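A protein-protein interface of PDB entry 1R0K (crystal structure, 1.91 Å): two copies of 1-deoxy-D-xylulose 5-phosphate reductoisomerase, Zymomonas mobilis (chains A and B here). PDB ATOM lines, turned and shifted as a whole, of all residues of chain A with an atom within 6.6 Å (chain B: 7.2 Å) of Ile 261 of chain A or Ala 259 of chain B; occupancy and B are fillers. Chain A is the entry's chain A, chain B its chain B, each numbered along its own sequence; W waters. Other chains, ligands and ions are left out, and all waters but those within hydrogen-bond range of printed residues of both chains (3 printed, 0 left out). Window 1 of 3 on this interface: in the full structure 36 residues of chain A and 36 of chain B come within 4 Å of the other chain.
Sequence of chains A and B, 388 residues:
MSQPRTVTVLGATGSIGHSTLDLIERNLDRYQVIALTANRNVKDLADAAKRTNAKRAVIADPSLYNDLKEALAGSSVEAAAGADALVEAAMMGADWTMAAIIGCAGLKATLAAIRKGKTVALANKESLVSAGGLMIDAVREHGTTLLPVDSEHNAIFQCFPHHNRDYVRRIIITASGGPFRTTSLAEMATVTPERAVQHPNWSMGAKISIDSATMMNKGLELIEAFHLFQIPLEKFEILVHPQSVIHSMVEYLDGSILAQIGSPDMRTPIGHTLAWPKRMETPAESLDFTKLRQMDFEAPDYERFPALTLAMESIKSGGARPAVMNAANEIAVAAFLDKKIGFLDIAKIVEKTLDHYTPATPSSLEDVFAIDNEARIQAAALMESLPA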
ATOM      1  N   ALA A 155      17.078   1.173  13.921  1.00  0.00           N
ATOM      2  CA  ALA A 155      17.014   1.036  12.475  1.00  0.00           C
ATOM      3  C   ALA A 155      17.780   2.207  11.845  1.00  0.00           C
ATOM      4  O   ALA A 155      18.592   2.019  10.940  1.00  0.00           O
ATOM      5  CB  ALA A 155      15.559   1.043  12.019  1.00  0.00           C
ATOM      6  N   CYS A 159      21.548   2.511   9.640  1.00  0.00           N
ATOM      7  CA  CYS A 159      21.594   3.071   8.286  1.00  0.00           C
ATOM      8  C   CYS A 159      22.224   4.459   8.265  1.00  0.00           C
ATOM      9  O   CYS A 159      22.266   5.112   7.219  1.00  0.00           O
ATOM     10  CB  CYS A 159      20.175   3.189   7.726  1.00  0.00           C
ATOM     11  SG  CYS A 159      19.232   1.658   7.691  1.00  0.00           S
ATOM     12  N   HIS A 241       3.454   3.581   7.600  1.00  0.00           N
ATOM     13  CA  HIS A 241       3.731   2.321   6.929  1.00  0.00           C
ATOM     14  C   HIS A 241       3.091   1.229   7.790  1.00  0.00           C
ATOM     15  O   HIS A 241       3.721   0.667   8.685  1.00  0.00           O
ATOM     16  CB  HIS A 241       5.257   2.157   6.819  1.00  0.00           C
ATOM     17  CG  HIS A 241       5.708   0.763   6.519  1.00  0.00           C
ATOM     18  ND1 HIS A 241       5.212   0.027   5.463  1.00  0.00           N
ATOM     19  CD2 HIS A 241       6.625  -0.025   7.129  1.00  0.00           C
ATOM     20  CE1 HIS A 241       5.805  -1.154   5.438  1.00  0.00           C
ATOM     21  NE2 HIS A 241       6.667  -1.210   6.438  1.00  0.00           N
ATOM     22  N   VAL A 245       7.298  -3.204   8.809  1.00  0.00           N
ATOM     23  CA  VAL A 245       8.439  -4.080   8.562  1.00  0.00           C
ATOM     24  C   VAL A 245       9.686  -3.239   8.294  1.00  0.00           C
ATOM     25  O   VAL A 245      10.769  -3.594   8.738  1.00  0.00           O
ATOM     26  CB  VAL A 245       8.179  -5.064   7.409  1.00  0.00           C
ATOM     27  CG1 VAL A 245       7.174  -6.118   7.870  1.00  0.00           C
ATOM     28  CG2 VAL A 245       7.667  -4.328   6.183  1.00  0.00           C
ATOM     29  N   ILE A 246       9.537  -2.132   7.567  1.00  0.00           N
ATOM     30  CA  ILE A 246      10.663  -1.219   7.359  1.00  0.00           C
ATOM     31  C   ILE A 246      10.605  -0.423   8.665  1.00  0.00           C
ATOM     32  O   ILE A 246       9.619   0.263   8.935  1.00  0.00           O
ATOM     33  CB  ILE A 246      10.443  -0.245   6.180  1.00  0.00           C
ATOM     34  CG1 ILE A 246      10.444  -1.006   4.853  1.00  0.00           C
ATOM     35  CG2 ILE A 246      11.543   0.807   6.172  1.00  0.00           C
ATOM     36  CD1 ILE A 246      10.315  -0.097   3.629  1.00  0.00           C
ATOM     37  N   HIS A 247      11.656  -0.517   9.470  1.00  0.00           N
ATOM     38  CA  HIS A 247      11.671   0.134  10.780  1.00  0.00           C
ATOM     39  C   HIS A 247      12.097   1.607  10.841  1.00  0.00           C
ATOM     40  O   HIS A 247      11.960   2.253  11.885  1.00  0.00           O
ATOM     41  CB  HIS A 247      12.501  -0.736  11.730  1.00  0.00           C
ATOM     42  CG  HIS A 247      11.956  -2.126  11.886  1.00  0.00           C
ATOM     43  ND1 HIS A 247      12.760  -3.243  11.942  1.00  0.00           N
ATOM     44  CD2 HIS A 247      10.681  -2.577  11.985  1.00  0.00           C
ATOM     45  CE1 HIS A 247      12.005  -4.323  12.061  1.00  0.00           C
ATOM     46  NE2 HIS A 247      10.740  -3.947  12.090  1.00  0.00           N
ATOM     47  N   SER A 248      12.581   2.118   9.709  1.00  0.00           N
ATOM     48  CA  SER A 248      13.013   3.508   9.507  1.00  0.00           C
ATOM     49  C   SER A 248      14.091   3.549   8.424  1.00  0.00           C
ATOM     50  O   SER A 248      14.662   2.515   8.083  1.00  0.00           O
ATOM     51  CB  SER A 248      13.513   4.151  10.804  1.00  0.00           C
ATOM     52  OG  SER A 248      12.410   4.610  11.575  1.00  0.00           O
ATOM     53  N   ILE A 257      18.918   5.419  -0.408  1.00  0.00           N
ATOM     54  CA  ILE A 257      18.154   5.322   0.831  1.00  0.00           C
ATOM     55  C   ILE A 257      18.463   3.985   1.493  1.00  0.00           C
ATOM     56  O   ILE A 257      18.238   2.921   0.908  1.00  0.00           O
ATOM     57  CB  ILE A 257      16.632   5.409   0.574  1.00  0.00           C
ATOM     58  CG1 ILE A 257      16.294   6.734  -0.112  1.00  0.00           C
ATOM     59  CG2 ILE A 257      15.869   5.284   1.896  1.00  0.00           C
ATOM     60  CD1 ILE A 257      14.824   6.861  -0.536  1.00  0.00           C
ATOM     61  N   LEU A 258      19.004   4.036   2.702  1.00  0.00           N
ATOM     62  CA  LEU A 258      19.307   2.811   3.421  1.00  0.00           C
ATOM     63  C   LEU A 258      18.200   2.588   4.433  1.00  0.00           C
ATOM     64  O   LEU A 258      17.847   3.493   5.186  1.00  0.00           O
ATOM     65  CB  LEU A 258      20.659   2.909   4.127  1.00  0.00           C
ATOM     66  CG  LEU A 258      21.873   3.107   3.214  1.00  0.00           C
ATOM     67  CD1 LEU A 258      23.148   2.947   4.033  1.00  0.00           C
ATOM     68  CD2 LEU A 258      21.841   2.103   2.070  1.00  0.00           C
ATOM     69  N   ALA A 259      17.655   1.378   4.436  1.00  0.00           N
ATOM     70  CA  ALA A 259      16.574   1.029   5.339  1.00  0.00           C
ATOM     71  C   ALA A 259      16.903  -0.235   6.114  1.00  0.00           C
ATOM     72  O   ALA A 259      17.671  -1.083   5.651  1.00  0.00           O
ATOM     73  CB  ALA A 259      15.290   0.822   4.549  1.00  0.00           C
ATOM     74  N   GLN A 260      16.329  -0.344   7.305  1.00  0.00           N
ATOM     75  CA  GLN A 260      16.509  -1.525   8.142  1.00  0.00           C
ATOM     76  C   GLN A 260      15.126  -2.153   8.185  1.00  0.00           C
ATOM     77  O   GLN A 260      14.155  -1.508   8.583  1.00  0.00           O
ATOM     78  CB  GLN A 260      16.979  -1.138   9.546  1.00  0.00           C
ATOM     79  CG  GLN A 260      17.524  -2.316  10.360  1.00  0.00           C
ATOM     80  CD  GLN A 260      16.430  -3.143  11.029  1.00  0.00           C
ATOM     81  OE1 GLN A 260      16.692  -4.221  11.570  1.00  0.00           O
ATOM     82  NE2 GLN A 260      15.206  -2.633  11.008  1.00  0.00           N
ATOM     83  N   ILE A 261      15.044  -3.407   7.757  1.00  0.00           N
ATOM     84  CA  ILE A 261      13.778  -4.121   7.689  1.00  0.00           C
ATOM     85  C   ILE A 261      13.882  -5.425   8.459  1.00  0.00           C
ATOM     86  O   ILE A 261      14.979  -5.932   8.682  1.00  0.00           O
ATOM     87  CB  ILE A 261      13.432  -4.452   6.211  1.00  0.00           C
ATOM     88  CG1 ILE A 261      13.620  -3.197   5.348  1.00  0.00           C
ATOM     89  CG2 ILE A 261      11.991  -4.983   6.105  1.00  0.00           C
ATOM     90  CD1 ILE A 261      13.427  -3.414   3.857  1.00  0.00           C
ATOM     91  N   GLY A 262      12.740  -5.962   8.876  1.00  0.00           N
ATOM     92  CA  GLY A 262      12.761  -7.225   9.587  1.00  0.00           C
ATOM     93  C   GLY A 262      11.503  -7.547  10.364  1.00  0.00           C
ATOM     94  O   GLY A 262      10.504  -6.822  10.308  1.00  0.00           O
ATOM     95  N   SER A 263      11.554  -8.669  11.074  1.00  0.00           N
ATOM     96  CA  SER A 263      10.452  -9.109  11.916  1.00  0.00           C
ATOM     97  C   SER A 263      10.455  -8.144  13.103  1.00  0.00           C
ATOM     98  O   SER A 263      11.418  -7.398  13.293  1.00  0.00           O
ATOM     99  CB  SER A 263      10.692 -10.546  12.390  1.00  0.00           C
ATOM    100  OG  SER A 263      11.908 -10.649  13.119  1.00  0.00           O
ATOM    101  N   THR A 268      16.432  -8.422  17.798  1.00  0.00           N
ATOM    102  CA  THR A 268      17.236  -7.992  16.656  1.00  0.00           C
ATOM    103  C   THR A 268      17.945  -6.679  17.013  1.00  0.00           C
ATOM    104  O   THR A 268      19.179  -6.609  16.990  1.00  0.00           O
ATOM    105  CB  THR A 268      16.366  -7.808  15.385  1.00  0.00           C
ATOM    106  OG1 THR A 268      15.891  -9.087  14.946  1.00  0.00           O
ATOM    107  CG2 THR A 268      17.193  -7.178  14.262  1.00  0.00           C
ATOM    108  N   LEU A 287      12.354 -12.215   8.102  1.00  0.00           N
ATOM    109  CA  LEU A 287      11.147 -11.734   7.441  1.00  0.00           C
ATOM    110  C   LEU A 287      10.901 -12.437   6.117  1.00  0.00           C
ATOM    111  O   LEU A 287      11.780 -12.488   5.259  1.00  0.00           O
ATOM    112  CB  LEU A 287      11.230 -10.224   7.206  1.00  0.00           C
ATOM    113  CG  LEU A 287       9.970  -9.600   6.605  1.00  0.00           C
ATOM    114  CD1 LEU A 287       8.817  -9.781   7.571  1.00  0.00           C
ATOM    115  CD2 LEU A 287      10.201  -8.123   6.313  1.00  0.00           C
ATOM    116  N   PHE A 289       9.263 -12.120   2.883  1.00  0.00           N
ATOM    117  CA  PHE A 289       8.640 -11.140   2.005  1.00  0.00           C
ATOM    118  C   PHE A 289       7.520 -11.713   1.154  1.00  0.00           C
ATOM    119  O   PHE A 289       6.557 -11.006   0.843  1.00  0.00           O
ATOM    120  CB  PHE A 289       9.685 -10.486   1.098  1.00  0.00           C
ATOM    121  CG  PHE A 289      10.681  -9.641   1.834  1.00  0.00           C
ATOM    122  CD1 PHE A 289      11.805 -10.213   2.420  1.00  0.00           C
ATOM    123  CD2 PHE A 289      10.490  -8.265   1.950  1.00  0.00           C
ATOM    124  CE1 PHE A 289      12.728  -9.426   3.113  1.00  0.00           C
ATOM    125  CE2 PHE A 289      11.407  -7.469   2.642  1.00  0.00           C
ATOM    126  CZ  PHE A 289      12.525  -8.049   3.223  1.00  0.00           C
ATOM    127  N   LEU A 292       4.607 -11.741   3.336  1.00  0.00           N
ATOM    128  CA  LEU A 292       4.230 -10.357   3.616  1.00  0.00           C
ATOM    129  C   LEU A 292       3.407  -9.871   2.428  1.00  0.00           C
ATOM    130  O   LEU A 292       2.364  -9.238   2.589  1.00  0.00           O
ATOM    131  CB  LEU A 292       5.477  -9.488   3.760  1.00  0.00           C
ATOM    132  CG  LEU A 292       5.262  -7.975   3.851  1.00  0.00           C
ATOM    133  CD1 LEU A 292       4.450  -7.624   5.095  1.00  0.00           C
ATOM    134  CD2 LEU A 292       6.626  -7.287   3.879  1.00  0.00           C
ATOM    135  N   MET A 295       3.674  -3.932   1.014  1.00  0.00           N
ATOM    136  CA  MET A 295       4.098  -2.884   1.941  1.00  0.00           C
ATOM    137  C   MET A 295       3.382  -1.619   1.491  1.00  0.00           C
ATOM    138  O   MET A 295       3.413  -1.279   0.308  1.00  0.00           O
ATOM    139  CB  MET A 295       5.602  -2.628   1.857  1.00  0.00           C
ATOM    140  CG  MET A 295       6.482  -3.612   2.595  1.00  0.00           C
ATOM    141  SD  MET A 295       8.213  -3.123   2.421  1.00  0.00           S
ATOM    142  CE  MET A 295       9.057  -4.634   2.943  1.00  0.00           C
ATOM    143  N   ALA B 155      23.569  -2.023  -4.569  1.00  0.00           N
ATOM    144  CA  ALA B 155      22.648  -2.033  -3.436  1.00  0.00           C
ATOM    145  C   ALA B 155      23.140  -3.054  -2.414  1.00  0.00           C
ATOM    146  O   ALA B 155      23.143  -2.794  -1.209  1.00  0.00           O
ATOM    147  CB  ALA B 155      21.244  -2.402  -3.910  1.00  0.00           C
ATOM    148  N   GLN B 158      26.244  -1.750  -0.609  1.00  0.00           N
ATOM    149  CA  GLN B 158      25.955  -0.739   0.412  1.00  0.00           C
ATOM    150  C   GLN B 158      25.347  -1.321   1.691  1.00  0.00           C
ATOM    151  O   GLN B 158      25.321  -0.661   2.720  1.00  0.00           O
ATOM    152  CB  GLN B 158      25.016   0.340  -0.145  1.00  0.00           C
ATOM    153  CG  GLN B 158      25.651   1.221  -1.225  1.00  0.00           C
ATOM    154  CD  GLN B 158      24.810   2.437  -1.574  1.00  0.00           C
ATOM    155  OE1 GLN B 158      24.277   3.110  -0.690  1.00  0.00           O
ATOM    156  NE2 GLN B 158      24.704   2.740  -2.868  1.00  0.00           N
ATOM    157  N   CYS B 159      24.863  -2.556   1.617  1.00  0.00           N
ATOM    158  CA  CYS B 159      24.248  -3.222   2.763  1.00  0.00           C
ATOM    159  C   CYS B 159      25.060  -4.425   3.248  1.00  0.00           C
ATOM    160  O   CYS B 159      24.645  -5.114   4.179  1.00  0.00           O
ATOM    161  CB  CYS B 159      22.849  -3.723   2.387  1.00  0.00           C
ATOM    162  SG  CYS B 159      21.712  -2.460   1.777  1.00  0.00           S
ATOM    163  N   ILE B 246      13.148  -1.268  -4.138  1.00  0.00           N
ATOM    164  CA  ILE B 246      14.113  -1.862  -3.220  1.00  0.00           C
ATOM    165  C   ILE B 246      15.035  -2.540  -4.227  1.00  0.00           C
ATOM    166  O   ILE B 246      14.617  -3.447  -4.962  1.00  0.00           O
ATOM    167  CB  ILE B 246      13.478  -2.912  -2.281  1.00  0.00           C
ATOM    168  CG1 ILE B 246      12.551  -2.207  -1.285  1.00  0.00           C
ATOM    169  CG2 ILE B 246      14.575  -3.688  -1.551  1.00  0.00           C
ATOM    170  CD1 ILE B 246      11.931  -3.118  -0.244  1.00  0.00           C
ATOM    171  N   HIS B 247      16.276  -2.077  -4.278  1.00  0.00           N
ATOM    172  CA  HIS B 247      17.244  -2.570  -5.247  1.00  0.00           C
ATOM    173  C   HIS B 247      17.972  -3.870  -4.898  1.00  0.00           C
ATOM    174  O   HIS B 247      18.622  -4.455  -5.762  1.00  0.00           O
ATOM    175  CB  HIS B 247      18.217  -1.435  -5.566  1.00  0.00           C
ATOM    176  CG  HIS B 247      17.541  -0.229  -6.148  1.00  0.00           C
ATOM    177  ND1 HIS B 247      17.885   1.061  -5.805  1.00  0.00           N
ATOM    178  CD2 HIS B 247      16.519  -0.124  -7.033  1.00  0.00           C
ATOM    179  CE1 HIS B 247      17.101   1.909  -6.449  1.00  0.00           C
ATOM    180  NE2 HIS B 247      16.264   1.216  -7.200  1.00  0.00           N
ATOM    181  N   SER B 248      17.829  -4.305  -3.646  1.00  0.00           N
ATOM    182  CA  SER B 248      18.378  -5.558  -3.107  1.00  0.00           C
ATOM    183  C   SER B 248      18.601  -5.462  -1.602  1.00  0.00           C
ATOM    184  O   SER B 248      18.592  -4.373  -1.032  1.00  0.00           O
ATOM    185  CB  SER B 248      19.666  -5.990  -3.816  1.00  0.00           C
ATOM    186  OG  SER B 248      19.340  -6.699  -5.006  1.00  0.00           O
ATOM    187  N   MET B 249      18.797  -6.604  -0.949  1.00  0.00           N
ATOM    188  CA  MET B 249      18.951  -6.588   0.497  1.00  0.00           C
ATOM    189  C   MET B 249      19.927  -7.624   1.037  1.00  0.00           C
ATOM    190  O   MET B 249      20.287  -8.586   0.349  1.00  0.00           O
ATOM    191  CB  MET B 249      17.582  -6.817   1.144  1.00  0.00           C
ATOM    192  CG  MET B 249      16.454  -6.006   0.528  1.00  0.00           C
ATOM    193  SD  MET B 249      14.847  -6.343   1.303  1.00  0.00           S
ATOM    194  CE  MET B 249      14.136  -7.483   0.135  1.00  0.00           C
ATOM    195  N   VAL B 250      20.334  -7.418   2.287  1.00  0.00           N
ATOM    196  CA  VAL B 250      21.244  -8.333   2.967  1.00  0.00           C
ATOM    197  C   VAL B 250      20.744  -8.556   4.390  1.00  0.00           C
ATOM    198  O   VAL B 250      20.555  -7.594   5.144  1.00  0.00           O
ATOM    199  CB  VAL B 250      22.684  -7.763   3.060  1.00  0.00           C
ATOM    200  CG1 VAL B 250      23.570  -8.732   3.828  1.00  0.00           C
ATOM    201  CG2 VAL B 250      23.255  -7.519   1.672  1.00  0.00           C
ATOM    202  N   GLU B 251      20.513  -9.811   4.762  1.00  0.00           N
ATOM    203  CA  GLU B 251      20.069 -10.092   6.122  1.00  0.00           C
ATOM    204  C   GLU B 251      21.256 -10.560   6.946  1.00  0.00           C
ATOM    205  O   GLU B 251      22.067 -11.370   6.489  1.00  0.00           O
ATOM    206  CB  GLU B 251      18.983 -11.172   6.167  1.00  0.00           C
ATOM    207  CG  GLU B 251      18.384 -11.327   7.572  1.00  0.00           C
ATOM    208  CD  GLU B 251      17.382 -12.456   7.677  1.00  0.00           C
ATOM    209  OE1 GLU B 251      16.541 -12.599   6.770  1.00  0.00           O
ATOM    210  OE2 GLU B 251      17.428 -13.196   8.683  1.00  0.00           O
ATOM    211  N   GLY B 255      19.010 -11.059  12.426  1.00  0.00           N
ATOM    212  CA  GLY B 255      17.676 -10.911  11.877  1.00  0.00           C
ATOM    213  C   GLY B 255      17.489  -9.599  11.145  1.00  0.00           C
ATOM    214  O   GLY B 255      16.486  -9.391  10.460  1.00  0.00           O
ATOM    215  N   SER B 256      18.466  -8.712  11.286  1.00  0.00           N
ATOM    216  CA  SER B 256      18.402  -7.412  10.642  1.00  0.00           C
ATOM    217  C   SER B 256      18.584  -7.518   9.131  1.00  0.00           C
ATOM    218  O   SER B 256      19.463  -8.223   8.637  1.00  0.00           O
ATOM    219  CB  SER B 256      19.469  -6.488  11.226  1.00  0.00           C
ATOM    220  OG  SER B 256      19.501  -5.255  10.534  1.00  0.00           O
ATOM    221  N   ILE B 257      17.726  -6.830   8.396  1.00  0.00           N
ATOM    222  CA  ILE B 257      17.832  -6.835   6.949  1.00  0.00           C
ATOM    223  C   ILE B 257      18.088  -5.400   6.516  1.00  0.00           C
ATOM    224  O   ILE B 257      17.286  -4.505   6.790  1.00  0.00           O
ATOM    225  CB  ILE B 257      16.540  -7.340   6.287  1.00  0.00           C
ATOM    226  CG1 ILE B 257      16.285  -8.795   6.693  1.00  0.00           C
ATOM    227  CG2 ILE B 257      16.664  -7.230   4.768  1.00  0.00           C
ATOM    228  CD1 ILE B 257      14.931  -9.329   6.259  1.00  0.00           C
ATOM    229  N   LEU B 258      19.226  -5.179   5.873  1.00  0.00           N
ATOM    230  CA  LEU B 258      19.565  -3.851   5.387  1.00  0.00           C
ATOM    231  C   LEU B 258      19.216  -3.838   3.910  1.00  0.00           C
ATOM    232  O   LEU B 258      19.559  -4.759   3.176  1.00  0.00           O
ATOM    233  CB  LEU B 258      21.056  -3.563   5.585  1.00  0.00           C
ATOM    234  CG  LEU B 258      21.507  -3.509   7.047  1.00  0.00           C
ATOM    235  CD1 LEU B 258      22.982  -3.127   7.126  1.00  0.00           C
ATOM    236  CD2 LEU B 258      20.645  -2.498   7.802  1.00  0.00           C
ATOM    237  N   ALA B 259      18.520  -2.797   3.481  1.00  0.00           N
ATOM    238  CA  ALA B 259      18.127  -2.695   2.087  1.00  0.00           C
ATOM    239  C   ALA B 259      18.526  -1.343   1.518  1.00  0.00           C
ATOM    240  O   ALA B 259      18.661  -0.364   2.252  1.00  0.00           O
ATOM    241  CB  ALA B 259      16.618  -2.887   1.964  1.00  0.00           C
ATOM    242  N   GLN B 260      18.746  -1.300   0.212  1.00  0.00           N
ATOM    243  CA  GLN B 260      19.080  -0.045  -0.440  1.00  0.00           C
ATOM    244  C   GLN B 260      17.865   0.226  -1.309  1.00  0.00           C
ATOM    245  O   GLN B 260      17.434  -0.636  -2.082  1.00  0.00           O
ATOM    246  CB  GLN B 260      20.346  -0.173  -1.284  1.00  0.00           C
ATOM    247  CG  GLN B 260      20.934   1.177  -1.715  1.00  0.00           C
ATOM    248  CD  GLN B 260      20.282   1.745  -2.971  1.00  0.00           C
ATOM    249  OE1 GLN B 260      20.501   2.911  -3.332  1.00  0.00           O
ATOM    250  NE2 GLN B 260      19.489   0.926  -3.646  1.00  0.00           N
ATOM    251  N   ILE B 261      17.301   1.417  -1.149  1.00  0.00           N
ATOM    252  CA  ILE B 261      16.101   1.818  -1.869  1.00  0.00           C
ATOM    253  C   ILE B 261      16.322   3.164  -2.546  1.00  0.00           C
ATOM    254  O   ILE B 261      17.139   3.959  -2.094  1.00  0.00           O
ATOM    255  CB  ILE B 261      14.913   1.946  -0.874  1.00  0.00           C
ATOM    256  CG1 ILE B 261      14.810   0.673  -0.027  1.00  0.00           C
ATOM    257  CG2 ILE B 261      13.608   2.194  -1.627  1.00  0.00           C
ATOM    258  CD1 ILE B 261      13.763   0.733   1.069  1.00  0.00           C
ATOM    259  N   MET B 295       4.300  -1.368  -2.366  1.00  0.00           N
ATOM    260  CA  MET B 295       5.382  -2.230  -2.842  1.00  0.00           C
ATOM    261  C   MET B 295       4.860  -3.665  -2.827  1.00  0.00           C
ATOM    262  O   MET B 295       4.205  -4.073  -1.872  1.00  0.00           O
ATOM    263  CB  MET B 295       6.607  -2.143  -1.920  1.00  0.00           C
ATOM    264  CG  MET B 295       7.521  -0.955  -2.160  1.00  0.00           C
ATOM    265  SD  MET B 295       8.873  -0.950  -0.975  1.00  0.00           S
ATOM    266  CE  MET B 295       9.327   0.796  -0.958  1.00  0.00           C
ATOM    267  N   PHE B 297       5.663  -7.970  -3.426  1.00  0.00           N
ATOM    268  CA  PHE B 297       6.698  -8.998  -3.388  1.00  0.00           C
ATOM    269  C   PHE B 297       6.080 -10.376  -3.617  1.00  0.00           C
ATOM    270  O   PHE B 297       4.988 -10.660  -3.135  1.00  0.00           O
ATOM    271  CB  PHE B 297       7.427  -8.996  -2.036  1.00  0.00           C
ATOM    272  CG  PHE B 297       7.969  -7.659  -1.644  1.00  0.00           C
ATOM    273  CD1 PHE B 297       7.182  -6.761  -0.928  1.00  0.00           C
ATOM    274  CD2 PHE B 297       9.260  -7.284  -2.007  1.00  0.00           C
ATOM    275  CE1 PHE B 297       7.674  -5.505  -0.580  1.00  0.00           C
ATOM    276  CE2 PHE B 297       9.762  -6.033  -1.667  1.00  0.00           C
ATOM    277  CZ  PHE B 297       8.968  -5.140  -0.951  1.00  0.00           C
HETATM  278  O   HOH W   1      20.674  -0.377   4.873  1.00  0.00           O
HETATM  279  O   HOH W   2      14.279  -8.679  12.863  1.00  0.00           O
HETATM  280  O   HOH W   3      14.001 -10.485   9.941  1.00  0.00           O
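ND1 of His 247 of chain B sits at hydrogen-bond distance from NE2 of Gln 260 of chain B (2.7 Å).
O of Val 250 of chain B sits at hydrogen-bond distance from N of Leu 258 of chain B (2.9 Å).
The backbone carbonyl oxygen (O) of Ser 248 of chain B sits at hydrogen-bond distance from the backbone NH (N) of Gln 260 of chain B, 3.3 Å away.
The backbone NH of Ala 259 of chain A sits close to the side-chain sulfur of Cys 159 of chain A, 3.6 Å away.
N of Gln 260 of chain A is in hydrogen-bond range of SG of Cys 159 of chain A.
N of Gln 260 of chain B is in hydrogen-bond range of SG of Cys 159 of chain B (3.5 Å).
Water W2 lies within hydrogen-bond range of OG1 of Thr 268 of chain A (2.7 Å), OG of Ser 263 of chain A (3.1 Å) and O of Gly 255 of chain B (3.3 Å).
Water W3 lies within hydrogen-bond range of O of Gly 255 of chain B, N of Leu 287 of chain A and N of Ser 263 of chain A.
Water W1 lies within hydrogen-bond range of O of Ala 259 of chain A (3.2 Å), O of Ala 259 of chain B (3.3 Å) and SG of Cys 159 of chain A (3.8 Å).
Of the 18 printed residues of chain B, 11 touch a printed residue of chain A.
Printed residues of chain B that touch a printed residue of chain A: Gln 158, Met 249, Gly 255, Ser 256, Ile 257, Leu 258, Ala 259, Gln 260, Ile 261, Met 295 and Phe 297.
Hydrophobic or aromatic side chains of chain B within 4 Å of the printed part of chain A: Met 249, Ile 257, Leu 258, Ala 259, Ile 261, Met 295 and Phe 297.
The backbone NH (N) of Ala 259 of chain B sits at hydrogen-bond distance from the backbone carbonyl oxygen (O) of Ala 259 of chain A, at 2.9 Å.
N of Ile 261 of chain A is in hydrogen-bond range of O of Ile 257 of chain B (2.7 Å).
The side-chain amide oxygen of Gln 260 of chain A sits at hydrogen-bond distance from the side-chain hydroxyl of Ser 256 of chain B, at 3.2 Å.
The backbone NH (N) of Met 295 of chain B sits at hydrogen-bond distance from the backbone carbonyl oxygen (O) of Met 295 of chain A (2.8 Å).
The backbone carbonyl oxygen (O) of Ile 257 of chain A lies within hydrogen-bond range of the backbone NH (N) of Ile 261 of chain B (2.7 Å).
Among the printed residues, pairs that only touch across the chains: Ile 257 of chain A with Ala 259 of chain B, Ile 257 of chain A with Gln 260 of chain B, Leu 258 of chain A with Gln 158 of chain B, Leu 258 of chain A with Ala 259 of chain B, Ala 259 of chain A with Ile 257 of chain B, Ala 259 of chain A with Leu 258 of chain B, Ala 259 of chain A with Ile 261 of chain B, Gln 260 of chain A with Ile 257 of chain B, Ile 261 of chain A with Ser 256 of chain B, Ile 261 of chain A with Ala 259 of chain B, Thr 268 of chain A with Gly 255 of chain B, Thr 268 of chain A with Ser 256 of chain B, Leu 287 of chain A with Ile 257 of chain B, Phe 289 of chain A with Met 249 of chain B, Phe 289 of chain A with Ile 257 of chain B, Phe 289 of chain A with Phe 297 of chain B and Met 295 of chain A with Phe 297 of chain B.
Ile 257 of chain A touches Ala 259 of chain B, and with the chains exchanged Ala 259 of chain A touches Ile 257 of chain B.
Leu 258 of chain A touches Ala 259 of chain B, and with the chains exchanged Ala 259 of chain A touches Leu 258 of chain B.
Ala 259 of chain A touches Ile 261 of chain B, and with the chains exchanged Ile 261 of chain A touches Ala 259 of chain B.
Met 295 of chain B touches its own counterpart, Met 295 of chain A.
Of the 22 pairs that touch across the chains among the printed residues, 12 have their exchanged pair printed and touching as well.
Printed residues of chain B within 4 Å of Ile 261 of chain A: Ser 256, Ile 257 and Ala 259.
Ala 259 of chain B touches just these residues of chain A: Ile 257 (3.6 Å), Leu 258 (3.4 Å), Ala 259 (2.9 Å) and Ile 261 (3.7 Å).
Of the printed residues of chain A, Met 295 of chain B touches Met 295 (2.8 Å).
Printed residues of chain A within 4 Å of Ile 257 of chain B: Ala 259 (3.6 Å), Gln 260 (3.4 Å), Ile 261 (2.7 Å), Leu 287 (3.9 Å) and Phe 289 (3.8 Å).
Of the printed residues of chain B, Ile 257 of chain A touches Ala 259 (3.6 Å), Gln 260 (3.4 Å) and Ile 261 (2.7 Å).
Printed residues of chain A within 4 Å of Gly 255 of chain B: Thr 268 (3.96 Å).
The nearest residue of chain A that does not touch Ala 259 of chain B is Gln 260 of chain A (5.0 Å).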
